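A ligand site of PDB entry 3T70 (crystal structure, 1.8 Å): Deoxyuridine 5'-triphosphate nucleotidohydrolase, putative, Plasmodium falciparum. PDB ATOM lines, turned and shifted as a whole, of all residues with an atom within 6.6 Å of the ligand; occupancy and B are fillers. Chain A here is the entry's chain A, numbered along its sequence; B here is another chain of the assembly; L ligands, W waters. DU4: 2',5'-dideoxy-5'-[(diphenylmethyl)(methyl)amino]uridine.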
ATOM      1  N   PHE A  46       9.406 -33.094  14.070  1.00  0.00           N
ATOM      2  CA  PHE A  46       9.230 -31.662  14.301  1.00  0.00           C
ATOM      3  C   PHE A  46      10.400 -30.918  13.670  1.00  0.00           C
ATOM      4  O   PHE A  46      11.476 -30.750  14.261  1.00  0.00           O
ATOM      5  CB  PHE A  46       9.035 -31.386  15.796  1.00  0.00           C
ATOM      6  CG  PHE A  46       7.807 -32.043  16.351  1.00  0.00           C
ATOM      7  CD1 PHE A  46       7.851 -33.370  16.793  1.00  0.00           C
ATOM      8  CD2 PHE A  46       6.600 -31.369  16.390  1.00  0.00           C
ATOM      9  CE1 PHE A  46       6.706 -33.994  17.283  1.00  0.00           C
ATOM     10  CE2 PHE A  46       5.447 -31.986  16.871  1.00  0.00           C
ATOM     11  CZ  PHE A  46       5.505 -33.297  17.326  1.00  0.00           C
ATOM     12  N   LEU A  88       0.125 -21.512   9.289  1.00  0.00           N
ATOM     13  CA  LEU A  88       1.112 -22.294   8.590  1.00  0.00           C
ATOM     14  C   LEU A  88       0.372 -23.356   7.775  1.00  0.00           C
ATOM     15  O   LEU A  88      -0.183 -24.288   8.358  1.00  0.00           O
ATOM     16  CB  LEU A  88       2.094 -22.948   9.574  1.00  0.00           C
ATOM     17  CG  LEU A  88       3.259 -23.775   9.028  1.00  0.00           C
ATOM     18  CD1 LEU A  88       4.226 -22.961   8.161  1.00  0.00           C
ATOM     19  CD2 LEU A  88       4.031 -24.435  10.167  1.00  0.00           C
ATOM     20  N   LEU A 101       1.099 -32.621   7.073  1.00  0.00           N
ATOM     21  CA  LEU A 101       1.223 -31.751   8.252  1.00  0.00           C
ATOM     22  C   LEU A 101       0.331 -32.330   9.358  1.00  0.00           C
ATOM     23  O   LEU A 101      -0.895 -32.362   9.236  1.00  0.00           O
ATOM     24  CB  LEU A 101       0.856 -30.301   7.924  1.00  0.00           C
ATOM     25  CG  LEU A 101       1.480 -29.231   8.874  1.00  0.00           C
ATOM     26  CD1 LEU A 101       2.985 -29.154   8.735  1.00  0.00           C
ATOM     27  CD2 LEU A 101       0.838 -27.862   8.613  1.00  0.00           C
ATOM     28  N   ALA A 102       0.978 -32.768  10.435  1.00  0.00           N
ATOM     29  CA  ALA A 102       0.292 -33.525  11.480  1.00  0.00           C
ATOM     30  C   ALA A 102      -0.907 -32.765  12.070  1.00  0.00           C
ATOM     31  O   ALA A 102      -1.970 -33.342  12.248  1.00  0.00           O
ATOM     32  CB  ALA A 102       1.269 -33.938  12.562  1.00  0.00           C
ATOM     33  N   ASN A 103      -0.722 -31.479  12.367  1.00  0.00           N
ATOM     34  CA  ASN A 103      -1.791 -30.639  12.915  1.00  0.00           C
ATOM     35  C   ASN A 103      -2.725 -29.955  11.887  1.00  0.00           C
ATOM     36  O   ASN A 103      -3.476 -29.036  12.239  1.00  0.00           O
ATOM     37  CB  ASN A 103      -1.215 -29.642  13.941  1.00  0.00           C
ATOM     38  CG  ASN A 103      -0.101 -28.760  13.363  1.00  0.00           C
ATOM     39  OD1 ASN A 103       0.673 -29.169  12.496  1.00  0.00           O
ATOM     40  ND2 ASN A 103      -0.009 -27.535  13.888  1.00  0.00           N
ATOM     41  N   ILE A 105      -3.310 -27.553   9.863  1.00  0.00           N
ATOM     42  CA  ILE A 105      -2.919 -26.156   9.614  1.00  0.00           C
ATOM     43  C   ILE A 105      -2.436 -25.627  10.954  1.00  0.00           C
ATOM     44  O   ILE A 105      -3.133 -25.770  11.962  1.00  0.00           O
ATOM     45  CB  ILE A 105      -4.115 -25.273   9.153  1.00  0.00           C
ATOM     46  CG1 ILE A 105      -4.825 -25.856   7.893  1.00  0.00           C
ATOM     47  CG2 ILE A 105      -3.671 -23.786   9.020  1.00  0.00           C
ATOM     48  CD1 ILE A 105      -4.026 -25.786   6.573  1.00  0.00           C
ATOM     49  N   GLY A 106      -1.261 -25.025  10.965  1.00  0.00           N
ATOM     50  CA  GLY A 106      -0.653 -24.523  12.193  1.00  0.00           C
ATOM     51  C   GLY A 106      -1.208 -23.157  12.513  1.00  0.00           C
ATOM     52  O   GLY A 106      -1.376 -22.323  11.602  1.00  0.00           O
ATOM     53  N   LEU A 107      -1.535 -22.935  13.789  1.00  0.00           N
ATOM     54  CA  LEU A 107      -1.994 -21.634  14.241  1.00  0.00           C
ATOM     55  C   LEU A 107      -0.893 -20.994  15.092  1.00  0.00           C
ATOM     56  O   LEU A 107      -0.550 -21.502  16.180  1.00  0.00           O
ATOM     57  CB  LEU A 107      -3.303 -21.761  15.024  1.00  0.00           C
ATOM     58  CG  LEU A 107      -4.303 -20.605  15.031  1.00  0.00           C
ATOM     59  CD1 LEU A 107      -5.448 -20.932  15.990  1.00  0.00           C
ATOM     60  CD2 LEU A 107      -3.693 -19.248  15.352  1.00  0.00           C
ATOM     61  N   ILE A 108      -0.328 -19.901  14.602  1.00  0.00           N
ATOM     62  CA  ILE A 108       0.729 -19.199  15.326  1.00  0.00           C
ATOM     63  C   ILE A 108       0.084 -17.993  15.995  1.00  0.00           C
ATOM     64  O   ILE A 108      -0.336 -17.086  15.297  1.00  0.00           O
ATOM     65  CB  ILE A 108       1.885 -18.730  14.392  1.00  0.00           C
ATOM     66  CG1 ILE A 108       2.322 -19.824  13.389  1.00  0.00           C
ATOM     67  CG2 ILE A 108       3.077 -18.185  15.232  1.00  0.00           C
ATOM     68  CD1 ILE A 108       2.898 -21.088  14.018  1.00  0.00           C
ATOM     69  N   ASP A 109       0.009 -17.988  17.320  1.00  0.00           N
ATOM     70  CA  ASP A 109      -0.620 -16.863  18.042  1.00  0.00           C
ATOM     71  C   ASP A 109       0.232 -15.598  17.927  1.00  0.00           C
ATOM     72  O   ASP A 109       1.444 -15.682  17.800  1.00  0.00           O
ATOM     73  CB  ASP A 109      -0.829 -17.199  19.519  1.00  0.00           C
ATOM     74  CG  ASP A 109      -1.821 -18.326  19.734  1.00  0.00           C
ATOM     75  OD1 ASP A 109      -3.004 -18.207  19.303  1.00  0.00           O
ATOM     76  OD2 ASP A 109      -1.414 -19.342  20.343  1.00  0.00           O
ATOM     77  N   TYR A 112       3.655 -15.521  20.018  1.00  0.00           N
ATOM     78  CA  TYR A 112       4.679 -16.571  19.955  1.00  0.00           C
ATOM     79  C   TYR A 112       6.020 -16.033  19.428  1.00  0.00           C
ATOM     80  O   TYR A 112       6.084 -15.377  18.383  1.00  0.00           O
ATOM     81  CB  TYR A 112       4.182 -17.745  19.103  1.00  0.00           C
ATOM     82  CG  TYR A 112       5.165 -18.883  18.963  1.00  0.00           C
ATOM     83  CD1 TYR A 112       5.475 -19.712  20.060  1.00  0.00           C
ATOM     84  CD2 TYR A 112       5.772 -19.152  17.745  1.00  0.00           C
ATOM     85  CE1 TYR A 112       6.374 -20.775  19.930  1.00  0.00           C
ATOM     86  CE2 TYR A 112       6.663 -20.207  17.607  1.00  0.00           C
ATOM     87  CZ  TYR A 112       6.965 -21.007  18.691  1.00  0.00           C
ATOM     88  OH  TYR A 112       7.858 -22.049  18.526  1.00  0.00           O
ATOM     89  N   GLY A 114       8.924 -18.263  19.607  1.00  0.00           N
ATOM     90  CA  GLY A 114       9.770 -19.427  19.374  1.00  0.00           C
ATOM     91  C   GLY A 114      10.001 -19.679  17.890  1.00  0.00           C
ATOM     92  O   GLY A 114       9.407 -19.014  17.032  1.00  0.00           O
ATOM     93  N   GLU A 115      10.846 -20.651  17.576  1.00  0.00           N
ATOM     94  CA  GLU A 115      11.160 -20.992  16.189  1.00  0.00           C
ATOM     95  C   GLU A 115       9.928 -21.599  15.523  1.00  0.00           C
ATOM     96  O   GLU A 115       9.168 -22.309  16.171  1.00  0.00           O
ATOM     97  CB  GLU A 115      12.322 -21.981  16.164  1.00  0.00           C
ATOM     98  CG  GLU A 115      12.786 -22.427  14.792  1.00  0.00           C
ATOM     99  CD  GLU A 115      14.094 -23.217  14.880  1.00  0.00           C
ATOM    100  OE1 GLU A 115      14.726 -23.449  13.839  1.00  0.00           O
ATOM    101  OE2 GLU A 115      14.464 -23.609  16.001  1.00  0.00           O
ATOM    102  N   ILE A 116       9.733 -21.299  14.250  1.00  0.00           N
ATOM    103  CA  ILE A 116       8.609 -21.875  13.517  1.00  0.00           C
ATOM    104  C   ILE A 116       8.989 -23.303  13.121  1.00  0.00           C
ATOM    105  O   ILE A 116      10.052 -23.548  12.549  1.00  0.00           O
ATOM    106  CB  ILE A 116       8.191 -21.040  12.294  1.00  0.00           C
ATOM    107  CG1 ILE A 116       7.827 -19.607  12.738  1.00  0.00           C
ATOM    108  CG2 ILE A 116       7.014 -21.689  11.571  1.00  0.00           C
ATOM    109  CD1 ILE A 116       7.620 -18.643  11.592  1.00  0.00           C
ATOM    110  N   ILE A 117       8.101 -24.235  13.475  1.00  0.00           N
ATOM    111  CA  ILE A 117       8.318 -25.663  13.254  1.00  0.00           C
ATOM    112  C   ILE A 117       7.177 -26.264  12.419  1.00  0.00           C
ATOM    113  O   ILE A 117       6.014 -25.875  12.591  1.00  0.00           O
ATOM    114  CB  ILE A 117       8.455 -26.402  14.620  1.00  0.00           C
ATOM    115  CG1 ILE A 117       9.632 -25.829  15.415  1.00  0.00           C
ATOM    116  CG2 ILE A 117       8.628 -27.911  14.416  1.00  0.00           C
ATOM    117  CD1 ILE A 117       9.744 -26.292  16.849  1.00  0.00           C
ATOM    118  N   ALA A 118       7.523 -27.181  11.517  1.00  0.00           N
ATOM    119  CA  ALA A 118       6.512 -27.950  10.767  1.00  0.00           C
ATOM    120  C   ALA A 118       6.526 -29.385  11.294  1.00  0.00           C
ATOM    121  O   ALA A 118       7.566 -30.067  11.223  1.00  0.00           O
ATOM    122  CB  ALA A 118       6.826 -27.937   9.279  1.00  0.00           C
ATOM    123  N   ALA A 119       5.394 -29.825  11.835  1.00  0.00           N
ATOM    124  CA  ALA A 119       5.246 -31.192  12.325  1.00  0.00           C
ATOM    125  C   ALA A 119       4.850 -32.098  11.167  1.00  0.00           C
ATOM    126  O   ALA A 119       3.712 -32.057  10.702  1.00  0.00           O
ATOM    127  CB  ALA A 119       4.195 -31.233  13.445  1.00  0.00           C
ATOM    128  N   ARG A 160      13.881 -14.186  24.161  1.00  0.00           N
ATOM    129  CA  ARG A 160      13.235 -15.191  23.294  1.00  0.00           C
ATOM    130  C   ARG A 160      12.918 -14.570  21.925  1.00  0.00           C
ATOM    131  O   ARG A 160      12.984 -15.246  20.905  1.00  0.00           O
ATOM    132  CB  ARG A 160      11.975 -15.819  23.931  1.00  0.00           C
ATOM    133  CG  ARG A 160      11.481 -17.046  23.111  1.00  0.00           C
ATOM    134  CD  ARG A 160      10.384 -17.902  23.768  1.00  0.00           C
ATOM    135  NE  ARG A 160      10.430 -19.267  23.202  1.00  0.00           N
ATOM    136  CZ  ARG A 160       9.377 -20.066  23.029  1.00  0.00           C
ATOM    137  NH1 ARG A 160       9.545 -21.281  22.506  1.00  0.00           N
ATOM    138  NH2 ARG A 160       8.157 -19.669  23.349  1.00  0.00           N
ATOM    139  N   ARG B  91      -5.429 -28.837  17.912  1.00  0.00           N
ATOM    140  CA  ARG B  91      -4.410 -28.161  18.698  1.00  0.00           C
ATOM    141  C   ARG B  91      -3.059 -28.665  18.206  1.00  0.00           C
ATOM    142  O   ARG B  91      -2.963 -29.791  17.742  1.00  0.00           O
ATOM    143  CB  ARG B  91      -4.604 -28.429  20.199  1.00  0.00           C
ATOM    144  CG  ARG B  91      -5.911 -27.857  20.723  1.00  0.00           C
ATOM    145  CD  ARG B  91      -6.033 -28.023  22.223  1.00  0.00           C
ATOM    146  NE  ARG B  91      -5.096 -27.153  22.938  1.00  0.00           N
ATOM    147  CZ  ARG B  91      -4.125 -27.583  23.746  1.00  0.00           C
ATOM    148  NH1 ARG B  91      -3.944 -28.875  23.976  1.00  0.00           N
ATOM    149  NH2 ARG B  91      -3.345 -26.703  24.339  1.00  0.00           N
ATOM    150  N   SER B  92      -2.027 -27.830  18.290  1.00  0.00           N
ATOM    151  CA  SER B  92      -0.701 -28.226  17.805  1.00  0.00           C
ATOM    152  C   SER B  92      -0.186 -29.471  18.524  1.00  0.00           C
ATOM    153  O   SER B  92       0.507 -30.289  17.930  1.00  0.00           O
ATOM    154  CB  SER B  92       0.310 -27.068  17.911  1.00  0.00           C
ATOM    155  OG  SER B  92       0.661 -26.790  19.246  1.00  0.00           O
ATOM    156  N   SER B  93      -0.566 -29.621  19.807  1.00  0.00           N
ATOM    157  CA  SER B  93      -0.145 -30.765  20.618  1.00  0.00           C
ATOM    158  C   SER B  93      -0.693 -32.116  20.143  1.00  0.00           C
ATOM    159  O   SER B  93      -0.207 -33.163  20.585  1.00  0.00           O
ATOM    160  CB  SER B  93      -0.510 -30.562  22.095  1.00  0.00           C
ATOM    161  OG  SER B  93      -1.898 -30.330  22.249  1.00  0.00           O
ATOM    162  N   ILE B  94      -1.717 -32.098  19.278  1.00  0.00           N
ATOM    163  CA  ILE B  94      -2.262 -33.340  18.700  1.00  0.00           C
ATOM    164  C   ILE B  94      -1.192 -34.111  17.941  1.00  0.00           C
ATOM    165  O   ILE B  94      -1.253 -35.356  17.822  1.00  0.00           O
ATOM    166  CB  ILE B  94      -3.515 -33.086  17.794  1.00  0.00           C
ATOM    167  CG1 ILE B  94      -4.432 -34.318  17.788  1.00  0.00           C
ATOM    168  CG2 ILE B  94      -3.116 -32.659  16.356  1.00  0.00           C
ATOM    169  CD1 ILE B  94      -5.774 -34.111  17.046  1.00  0.00           C
ATOM    170  N   SER B  95      -0.200 -33.361  17.445  1.00  0.00           N
ATOM    171  CA  SER B  95       0.894 -33.909  16.643  1.00  0.00           C
ATOM    172  C   SER B  95       1.696 -34.934  17.436  1.00  0.00           C
ATOM    173  O   SER B  95       2.289 -35.842  16.846  1.00  0.00           O
ATOM    174  CB  SER B  95       1.809 -32.794  16.147  1.00  0.00           C
ATOM    175  OG  SER B  95       1.085 -31.775  15.473  1.00  0.00           O
ATOM    176  N   LYS B  96       1.699 -34.794  18.750  1.00  0.00           N
ATOM    177  CA  LYS B  96       2.425 -35.690  19.656  1.00  0.00           C
ATOM    178  C   LYS B  96       1.676 -37.004  19.884  1.00  0.00           C
ATOM    179  O   LYS B  96       2.228 -37.915  20.531  1.00  0.00           O
ATOM    180  CB  LYS B  96       2.705 -35.012  21.004  1.00  0.00           C
ATOM    181  CG  LYS B  96       3.485 -33.700  20.921  1.00  0.00           C
ATOM    182  CD  LYS B  96       3.867 -33.210  22.315  1.00  0.00           C
ATOM    183  CE  LYS B  96       4.392 -31.780  22.275  1.00  0.00           C
ATOM    184  NZ  LYS B  96       3.306 -30.767  22.042  1.00  0.00           N
HETATM  185  N1  DU4 L   1       3.701 -23.712  16.193  1.00  0.00           N
HETATM  186  C2  DU4 L   1       4.559 -24.042  15.134  1.00  0.00           C
HETATM  187  O2  DU4 L   1       5.744 -23.735  15.159  1.00  0.00           O
HETATM  188  N3  DU4 L   1       4.036 -24.719  14.031  1.00  0.00           N
HETATM  189  C4  DU4 L   1       2.682 -25.077  13.984  1.00  0.00           C
HETATM  190  O4  DU4 L   1       2.287 -25.678  12.991  1.00  0.00           O
HETATM  191  C5  DU4 L   1       1.826 -24.768  15.033  1.00  0.00           C
HETATM  192  C6  DU4 L   1       2.335 -24.075  16.142  1.00  0.00           C
HETATM  193  C1' DU4 L   1       4.295 -23.011  17.380  1.00  0.00           C
HETATM  194  C17 DU4 L   1       5.199 -27.947  19.284  1.00  0.00           C
HETATM  195  C18 DU4 L   1       6.451 -28.854  19.390  1.00  0.00           C
HETATM  196  C19 DU4 L   1       6.282 -30.174  19.837  1.00  0.00           C
HETATM  197  C2' DU4 L   1       3.329 -22.378  18.374  1.00  0.00           C
HETATM  198  C20 DU4 L   1       7.374 -31.032  19.956  1.00  0.00           C
HETATM  199  C21 DU4 L   1       8.639 -30.570  19.615  1.00  0.00           C
HETATM  200  C22 DU4 L   1       8.823 -29.266  19.163  1.00  0.00           C
HETATM  201  C23 DU4 L   1       7.722 -28.410  19.049  1.00  0.00           C
HETATM  202  C24 DU4 L   1       4.669 -28.011  17.837  1.00  0.00           C
HETATM  203  C25 DU4 L   1       3.552 -28.799  17.571  1.00  0.00           C
HETATM  204  C26 DU4 L   1       3.040 -28.891  16.271  1.00  0.00           C
HETATM  205  C27 DU4 L   1       3.645 -28.196  15.237  1.00  0.00           C
HETATM  206  C28 DU4 L   1       4.774 -27.414  15.497  1.00  0.00           C
HETATM  207  C29 DU4 L   1       5.294 -27.319  16.792  1.00  0.00           C
HETATM  208  C3' DU4 L   1       3.151 -23.429  19.452  1.00  0.00           C
HETATM  209  O3' DU4 L   1       3.056 -22.749  20.721  1.00  0.00           O
HETATM  210  C4' DU4 L   1       4.439 -24.244  19.416  1.00  0.00           C
HETATM  211  O4' DU4 L   1       5.008 -24.077  18.069  1.00  0.00           O
HETATM  212  C41 DU4 L   1       5.857 -26.537  21.189  1.00  0.00           C
HETATM  213  C5' DU4 L   1       4.156 -25.741  19.715  1.00  0.00           C
HETATM  214  N5' DU4 L   1       5.402 -26.552  19.772  1.00  0.00           N
HETATM  215  O   HOH W   1       7.822 -24.997  19.141  1.00  0.00           O
HETATM  216  O   HOH W   2      -1.526 -25.014  15.674  1.00  0.00           O
HETATM  217  O   HOH W   3       1.179 -19.934  19.031  1.00  0.00           O
HETATM  218  O   HOH W   4       0.712 -23.766  21.851  1.00  0.00           O
HETATM  219  O   HOH W   5       2.451 -28.610  21.221  1.00  0.00           O
HETATM  220  O   HOH W   6       3.153 -28.027  11.789  1.00  0.00           O
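The backbone NH (N) of Ile 117 lies within hydrogen-bond range of an oxygen (O2) of the ligand (2.9 Å). A nitrogen (N3) of the ligand sits at hydrogen-bond distance from the backbone carbonyl oxygen (O) of Ile 117 (2.7 Å). An oxygen (O4) of the ligand is in hydrogen-bond range of the side-chain amide nitrogen of Asn 103.
N of Leu 88 is in hydrogen-bond range of O of Gly 106, 2.9 Å away. O of Ser 92 of chain B sits at hydrogen-bond distance from OG of Ser 95 of chain B (2.9 Å). The side-chain hydroxyl (OH) of Tyr 112 sits at hydrogen-bond distance from the backbone carbonyl oxygen (O) of Glu 115. The backbone carbonyl oxygen of Ala 119 sits at hydrogen-bond distance from the backbone NH of Ala 102 (2.8 Å).
Phe 46 touches the ligand. Leu 88 touches the ligand (CD2 to O4, 3.5 Å). Gly 106 touches the ligand. O of Leu 107 touches C6 of the ligand, 3.9 Å away. CD1 of Ile 108 touches N1 of the ligand, at 3.5 Å. OH of Tyr 112 touches O4' of the ligand, 3.5 Å away. O of Glu 115 touches O2 of the ligand (3.8 Å). Ile 116 touches the ligand (CA to O2, 3.8 Å). Ala 119 touches the ligand. O of Ser 92 of chain B touches C26 of the ligand, at 3.3 Å. OG of Ser 95 of chain B touches C26 of the ligand, at 3.6 Å. Lys 96 of chain B touches the ligand (CE to C19, 3.5 Å). The nearest printed residue that does not touch the ligand is Ser 93 of chain B (4.8 Å).
Water W6 lies within hydrogen-bond range of an oxygen (O4) of the ligand (2.8 Å), the side-chain amide oxygen (OD1) of Asn 103 (2.8 Å) and the backbone NH (N) of Ala 119 (2.9 Å). Water W1 lies within hydrogen-bond range of OH of Tyr 112 and O4' of the ligand. Water W2 lies within hydrogen-bond range of N of Leu 107 and ND2 of Asn 103. Water W5 lies within hydrogen-bond range of NZ of Lys 96 of chain B (2.5 Å), OG of Ser 92 of chain B (3.2 Å) and N of Ser 93 of chain B (3.5 Å).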
